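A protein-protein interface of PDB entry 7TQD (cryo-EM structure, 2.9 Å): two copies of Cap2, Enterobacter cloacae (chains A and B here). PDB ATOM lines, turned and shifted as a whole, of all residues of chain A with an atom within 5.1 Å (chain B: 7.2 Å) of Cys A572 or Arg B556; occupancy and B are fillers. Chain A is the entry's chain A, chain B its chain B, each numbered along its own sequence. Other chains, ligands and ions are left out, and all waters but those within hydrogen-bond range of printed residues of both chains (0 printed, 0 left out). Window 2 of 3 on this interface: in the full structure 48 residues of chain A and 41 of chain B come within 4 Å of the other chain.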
ATOM      1  N   ILE A 376      23.643  27.188  18.092  1.00  0.00           N
ATOM      2  CA  ILE A 376      24.497  26.086  17.663  1.00  0.00           C
ATOM      3  C   ILE A 376      25.647  26.551  16.777  1.00  0.00           C
ATOM      4  O   ILE A 376      26.635  25.820  16.626  1.00  0.00           O
ATOM      5  CB  ILE A 376      23.678  25.005  16.932  1.00  0.00           C
ATOM      6  CG1 ILE A 376      24.407  23.660  16.974  1.00  0.00           C
ATOM      7  CG2 ILE A 376      23.399  25.416  15.497  1.00  0.00           C
ATOM      8  CD1 ILE A 376      23.662  22.542  16.291  1.00  0.00           C
ATOM      9  N   ILE A 400      25.283  24.814   6.980  1.00  0.00           N
ATOM     10  CA  ILE A 400      24.257  25.595   7.667  1.00  0.00           C
ATOM     11  C   ILE A 400      24.826  26.599   8.662  1.00  0.00           C
ATOM     12  O   ILE A 400      24.056  27.396   9.222  1.00  0.00           O
ATOM     13  CB  ILE A 400      23.229  24.692   8.383  1.00  0.00           C
ATOM     14  CG1 ILE A 400      23.850  24.026   9.609  1.00  0.00           C
ATOM     15  CG2 ILE A 400      22.651  23.666   7.422  1.00  0.00           C
ATOM     16  CD1 ILE A 400      22.868  23.197  10.401  1.00  0.00           C
ATOM     17  N   GLY A 567      19.014  13.529  10.989  1.00  0.00           N
ATOM     18  CA  GLY A 567      19.927  13.667  12.108  1.00  0.00           C
ATOM     19  C   GLY A 567      20.361  15.098  12.345  1.00  0.00           C
ATOM     20  O   GLY A 567      20.511  15.524  13.491  1.00  0.00           O
ATOM     21  N   THR A 568      20.581  15.859  11.272  1.00  0.00           N
ATOM     22  CA  THR A 568      20.931  17.265  11.445  1.00  0.00           C
ATOM     23  C   THR A 568      19.797  18.037  12.112  1.00  0.00           C
ATOM     24  O   THR A 568      20.032  18.847  13.023  1.00  0.00           O
ATOM     25  CB  THR A 568      21.288  17.891  10.098  1.00  0.00           C
ATOM     26  OG1 THR A 568      22.342  17.140   9.489  1.00  0.00           O
ATOM     27  CG2 THR A 568      21.749  19.322  10.286  1.00  0.00           C
ATOM     28  N   LYS A 569      18.555  17.793  11.680  1.00  0.00           N
ATOM     29  CA  LYS A 569      17.428  18.453  12.337  1.00  0.00           C
ATOM     30  C   LYS A 569      17.335  18.058  13.809  1.00  0.00           C
ATOM     31  O   LYS A 569      17.089  18.909  14.676  1.00  0.00           O
ATOM     32  CB  LYS A 569      16.123  18.139  11.612  1.00  0.00           C
ATOM     33  CG  LYS A 569      16.088  18.597  10.168  1.00  0.00           C
ATOM     34  CD  LYS A 569      14.782  18.210   9.500  1.00  0.00           C
ATOM     35  CE  LYS A 569      14.905  18.256   7.991  1.00  0.00           C
ATOM     36  NZ  LYS A 569      15.228  19.626   7.518  1.00  0.00           N
ATOM     37  N   PHE A 570      17.528  16.772  14.109  1.00  0.00           N
ATOM     38  CA  PHE A 570      17.480  16.315  15.494  1.00  0.00           C
ATOM     39  C   PHE A 570      18.567  16.975  16.331  1.00  0.00           C
ATOM     40  O   PHE A 570      18.330  17.352  17.484  1.00  0.00           O
ATOM     41  CB  PHE A 570      17.607  14.792  15.537  1.00  0.00           C
ATOM     42  CG  PHE A 570      17.679  14.222  16.922  1.00  0.00           C
ATOM     43  CD1 PHE A 570      16.526  13.951  17.632  1.00  0.00           C
ATOM     44  CD2 PHE A 570      18.900  13.938  17.509  1.00  0.00           C
ATOM     45  CE1 PHE A 570      16.585  13.421  18.902  1.00  0.00           C
ATOM     46  CE2 PHE A 570      18.964  13.407  18.780  1.00  0.00           C
ATOM     47  CZ  PHE A 570      17.805  13.149  19.478  1.00  0.00           C
ATOM     48  N   ILE A 571      19.768  17.119  15.769  1.00  0.00           N
ATOM     49  CA  ILE A 571      20.863  17.761  16.488  1.00  0.00           C
ATOM     50  C   ILE A 571      20.515  19.206  16.807  1.00  0.00           C
ATOM     51  O   ILE A 571      20.737  19.679  17.928  1.00  0.00           O
ATOM     52  CB  ILE A 571      22.169  17.662  15.676  1.00  0.00           C
ATOM     53  CG1 ILE A 571      22.703  16.232  15.696  1.00  0.00           C
ATOM     54  CG2 ILE A 571      23.209  18.631  16.210  1.00  0.00           C
ATOM     55  CD1 ILE A 571      23.816  15.989  14.710  1.00  0.00           C
ATOM     56  N   CYS A 572      19.968  19.933  15.830  1.00  0.00           N
ATOM     57  CA  CYS A 572      19.598  21.325  16.080  1.00  0.00           C
ATOM     58  C   CYS A 572      18.537  21.423  17.173  1.00  0.00           C
ATOM     59  O   CYS A 572      18.639  22.259  18.083  1.00  0.00           O
ATOM     60  CB  CYS A 572      19.110  21.979  14.789  1.00  0.00           C
ATOM     61  SG  CYS A 572      20.379  22.129  13.513  1.00  0.00           S
ATOM     62  N   ARG A 573      17.523  20.553  17.117  1.00  0.00           N
ATOM     63  CA  ARG A 573      16.474  20.586  18.131  1.00  0.00           C
ATOM     64  C   ARG A 573      17.027  20.290  19.519  1.00  0.00           C
ATOM     65  O   ARG A 573      16.648  20.942  20.497  1.00  0.00           O
ATOM     66  CB  ARG A 573      15.365  19.594  17.791  1.00  0.00           C
ATOM     67  CG  ARG A 573      14.486  20.000  16.632  1.00  0.00           C
ATOM     68  CD  ARG A 573      13.131  19.320  16.724  1.00  0.00           C
ATOM     69  NE  ARG A 573      13.239  17.870  16.815  1.00  0.00           N
ATOM     70  CZ  ARG A 573      13.304  17.057  15.771  1.00  0.00           C
ATOM     71  NH1 ARG A 573      13.286  17.520  14.531  1.00  0.00           N
ATOM     72  NH2 ARG A 573      13.384  15.746  15.974  1.00  0.00           N
ATOM     73  N   VAL A 574      17.917  19.301  19.626  1.00  0.00           N
ATOM     74  CA  VAL A 574      18.467  18.942  20.931  1.00  0.00           C
ATOM     75  C   VAL A 574      19.335  20.068  21.477  1.00  0.00           C
ATOM     76  O   VAL A 574      19.282  20.388  22.669  1.00  0.00           O
ATOM     77  CB  VAL A 574      19.246  17.618  20.839  1.00  0.00           C
ATOM     78  CG1 VAL A 574      20.140  17.445  22.049  1.00  0.00           C
ATOM     79  CG2 VAL A 574      18.285  16.458  20.721  1.00  0.00           C
ATOM     80  N   VAL A 575      20.141  20.693  20.616  1.00  0.00           N
ATOM     81  CA  VAL A 575      20.986  21.795  21.070  1.00  0.00           C
ATOM     82  C   VAL A 575      20.130  22.958  21.554  1.00  0.00           C
ATOM     83  O   VAL A 575      20.487  23.652  22.514  1.00  0.00           O
ATOM     84  CB  VAL A 575      21.958  22.225  19.955  1.00  0.00           C
ATOM     85  CG1 VAL A 575      22.644  23.531  20.314  1.00  0.00           C
ATOM     86  CG2 VAL A 575      22.985  21.141  19.717  1.00  0.00           C
ATOM     87  N   SER A 576      18.985  23.190  20.904  1.00  0.00           N
ATOM     88  CA  SER A 576      18.108  24.268  21.358  1.00  0.00           C
ATOM     89  C   SER A 576      17.598  24.022  22.777  1.00  0.00           C
ATOM     90  O   SER A 576      17.577  24.942  23.602  1.00  0.00           O
ATOM     91  CB  SER A 576      16.939  24.440  20.391  1.00  0.00           C
ATOM     92  OG  SER A 576      17.387  24.960  19.152  1.00  0.00           O
ATOM     93  N   MET B 392      22.109  17.500  -6.845  1.00  0.00           N
ATOM     94  CA  MET B 392      22.048  16.463  -5.821  1.00  0.00           C
ATOM     95  C   MET B 392      21.399  15.193  -6.357  1.00  0.00           C
ATOM     96  O   MET B 392      21.858  14.081  -6.064  1.00  0.00           O
ATOM     97  CB  MET B 392      21.296  16.977  -4.595  1.00  0.00           C
ATOM     98  CG  MET B 392      22.002  18.110  -3.874  1.00  0.00           C
ATOM     99  SD  MET B 392      21.022  18.791  -2.527  1.00  0.00           S
ATOM    100  CE  MET B 392      22.078  20.128  -1.979  1.00  0.00           C
ATOM    101  N   ARG B 505       9.530  28.155   1.070  1.00  0.00           N
ATOM    102  CA  ARG B 505      10.242  27.794   2.295  1.00  0.00           C
ATOM    103  C   ARG B 505      10.584  26.309   2.356  1.00  0.00           C
ATOM    104  O   ARG B 505      10.874  25.783   3.435  1.00  0.00           O
ATOM    105  CB  ARG B 505       9.449  28.197   3.544  1.00  0.00           C
ATOM    106  CG  ARG B 505       9.322  29.693   3.755  1.00  0.00           C
ATOM    107  CD  ARG B 505       8.742  29.996   5.126  1.00  0.00           C
ATOM    108  NE  ARG B 505       7.581  29.164   5.417  1.00  0.00           N
ATOM    109  CZ  ARG B 505       6.324  29.542   5.234  1.00  0.00           C
ATOM    110  NH1 ARG B 505       6.025  30.739   4.759  1.00  0.00           N
ATOM    111  NH2 ARG B 505       5.341  28.697   5.534  1.00  0.00           N
ATOM    112  N   ALA B 506      10.547  25.623   1.212  1.00  0.00           N
ATOM    113  CA  ALA B 506      10.916  24.211   1.116  1.00  0.00           C
ATOM    114  C   ALA B 506      10.110  23.348   2.082  1.00  0.00           C
ATOM    115  O   ALA B 506      10.618  22.380   2.648  1.00  0.00           O
ATOM    116  CB  ALA B 506      12.417  24.020   1.337  1.00  0.00           C
ATOM    117  N   ALA B 555      17.287  28.256   0.660  1.00  0.00           N
ATOM    118  CA  ALA B 555      16.793  27.421   1.748  1.00  0.00           C
ATOM    119  C   ALA B 555      17.934  26.664   2.417  1.00  0.00           C
ATOM    120  O   ALA B 555      19.050  26.625   1.902  1.00  0.00           O
ATOM    121  CB  ALA B 555      15.741  26.454   1.236  1.00  0.00           C
ATOM    122  N   ARG B 556      17.647  26.066   3.571  1.00  0.00           N
ATOM    123  CA  ARG B 556      18.655  25.295   4.285  1.00  0.00           C
ATOM    124  C   ARG B 556      19.068  24.070   3.479  1.00  0.00           C
ATOM    125  O   ARG B 556      18.265  23.486   2.747  1.00  0.00           O
ATOM    126  CB  ARG B 556      18.124  24.883   5.658  1.00  0.00           C
ATOM    127  CG  ARG B 556      18.117  26.015   6.666  1.00  0.00           C
ATOM    128  CD  ARG B 556      17.694  25.544   8.049  1.00  0.00           C
ATOM    129  NE  ARG B 556      18.507  24.442   8.546  1.00  0.00           N
ATOM    130  CZ  ARG B 556      18.291  23.815   9.695  1.00  0.00           C
ATOM    131  NH1 ARG B 556      17.299  24.163  10.497  1.00  0.00           N
ATOM    132  NH2 ARG B 556      19.088  22.811  10.048  1.00  0.00           N
ATOM    133  N   ALA B 557      20.340  23.690   3.615  1.00  0.00           N
ATOM    134  CA  ALA B 557      20.883  22.592   2.821  1.00  0.00           C
ATOM    135  C   ALA B 557      20.200  21.268   3.143  1.00  0.00           C
ATOM    136  O   ALA B 557      19.992  20.437   2.252  1.00  0.00           O
ATOM    137  CB  ALA B 557      22.390  22.485   3.044  1.00  0.00           C
ATOM    138  N   ASP B 558      19.858  21.045   4.416  1.00  0.00           N
ATOM    139  CA  ASP B 558      19.292  19.758   4.808  1.00  0.00           C
ATOM    140  C   ASP B 558      17.908  19.550   4.203  1.00  0.00           C
ATOM    141  O   ASP B 558      17.537  18.419   3.871  1.00  0.00           O
ATOM    142  CB  ASP B 558      19.243  19.640   6.331  1.00  0.00           C
ATOM    143  CG  ASP B 558      18.586  20.832   6.985  1.00  0.00           C
ATOM    144  OD1 ASP B 558      18.174  21.755   6.257  1.00  0.00           O
ATOM    145  OD2 ASP B 558      18.485  20.852   8.230  1.00  0.00           O
ATOM    146  N   ASP B 559      17.133  20.625   4.044  1.00  0.00           N
ATOM    147  CA  ASP B 559      15.841  20.507   3.373  1.00  0.00           C
ATOM    148  C   ASP B 559      16.015  20.070   1.925  1.00  0.00           C
ATOM    149  O   ASP B 559      15.304  19.182   1.434  1.00  0.00           O
ATOM    150  CB  ASP B 559      15.088  21.836   3.445  1.00  0.00           C
ATOM    151  CG  ASP B 559      14.953  22.353   4.858  1.00  0.00           C
ATOM    152  OD1 ASP B 559      15.078  21.546   5.800  1.00  0.00           O
ATOM    153  OD2 ASP B 559      14.715  23.566   5.026  1.00  0.00           O
ATOM    154  N   VAL B 560      16.971  20.685   1.225  1.00  0.00           N
ATOM    155  CA  VAL B 560      17.221  20.329  -0.167  1.00  0.00           C
ATOM    156  C   VAL B 560      17.696  18.888  -0.268  1.00  0.00           C
ATOM    157  O   VAL B 560      17.303  18.153  -1.179  1.00  0.00           O
ATOM    158  CB  VAL B 560      18.231  21.307  -0.798  1.00  0.00           C
ATOM    159  CG1 VAL B 560      18.319  21.078  -2.290  1.00  0.00           C
ATOM    160  CG2 VAL B 560      17.837  22.744  -0.501  1.00  0.00           C
ATOM    161  N   GLN B 561      18.544  18.457   0.670  1.00  0.00           N
ATOM    162  CA  GLN B 561      19.021  17.076   0.660  1.00  0.00           C
ATOM    163  C   GLN B 561      17.882  16.095   0.918  1.00  0.00           C
ATOM    164  O   GLN B 561      17.799  15.041   0.274  1.00  0.00           O
ATOM    165  CB  GLN B 561      20.126  16.903   1.700  1.00  0.00           C
ATOM    166  CG  GLN B 561      21.398  17.664   1.372  1.00  0.00           C
ATOM    167  CD  GLN B 561      22.332  16.890   0.468  1.00  0.00           C
ATOM    168  OE1 GLN B 561      21.982  15.828  -0.045  1.00  0.00           O
ATOM    169  NE2 GLN B 561      23.532  17.422   0.265  1.00  0.00           N
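Of the 12 printed residues of chain A, 3 touch a printed residue of chain B. Printed residues of chain A that touch a printed residue of chain B: Ile A400, Lys A569 and Cys A572. Hydrophobic or aromatic side chains of chain A within 4 Å of the printed part of chain B: Ile A400. Among the printed residues, 4 pairs touch across the chains. Among the printed residues, Asp or Glu carboxylates within 4 Å of a Lys or Arg side-chain nitrogen of the other chain: Lys A569 with Asp B558 (3.6 Å) and Lys A569 with Asp B559 (2.6 Å).
Cys A572 touches one residue of chain B. Arg B556 touches just these residues of chain A: Ile A400 and Cys A572. Printed residues of chain A within 4 Å of Asp B558: Lys A569 (3.6 Å). Printed residues of chain A within 4 Å of Asp B559: Lys A569. Printed residues of chain B within 4 Å of Lys A569: Asp B558 (3.6 Å) and Asp B559 (2.6 Å). Printed residues of chain B within 4 Å of Ile A400: Arg B556. The nearest residue of chain A that does not touch Arg B556 is Thr A568 (4.4 Å). The nearest printed residue of chain B that does not touch Ile A400 is Ala B557 (4.5 Å).
NH2 of Arg B556 touches CD1 of Ile A400, 3.8 Å away.
No position is printed for both chains. Of the 4 pairs that touch across the chains among the printed residues, none has its exchanged pair printed and touching as well.
The side-chain sulfur (SG) of Cys A572 is in hydrogen-bond range of the guanidinium group (NH2) of Arg B556 (3.8 Å). The side-chain carboxylate (OD1) of Asp B559 lies within salt-bridge range of the side-chain amino group (NZ) of Lys A569, at 2.6 Å. The side-chain carboxylate of Asp B558 is in salt-bridge range of the side-chain amino group of Lys A569 (3.6 Å).
The side-chain carboxylate (OD2) of Asp B558 is in salt-bridge range of the guanidinium group (NH2) of Arg B556 (2.7 Å). The backbone carbonyl oxygen (O) of Thr A568 sits at hydrogen-bond distance from the side-chain sulfur (SG) of Cys A572 (3.3 Å). The backbone carbonyl oxygen (O) of Cys A572 is in hydrogen-bond range of the side-chain hydroxyl (OG) of Ser A576 (3.2 Å).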
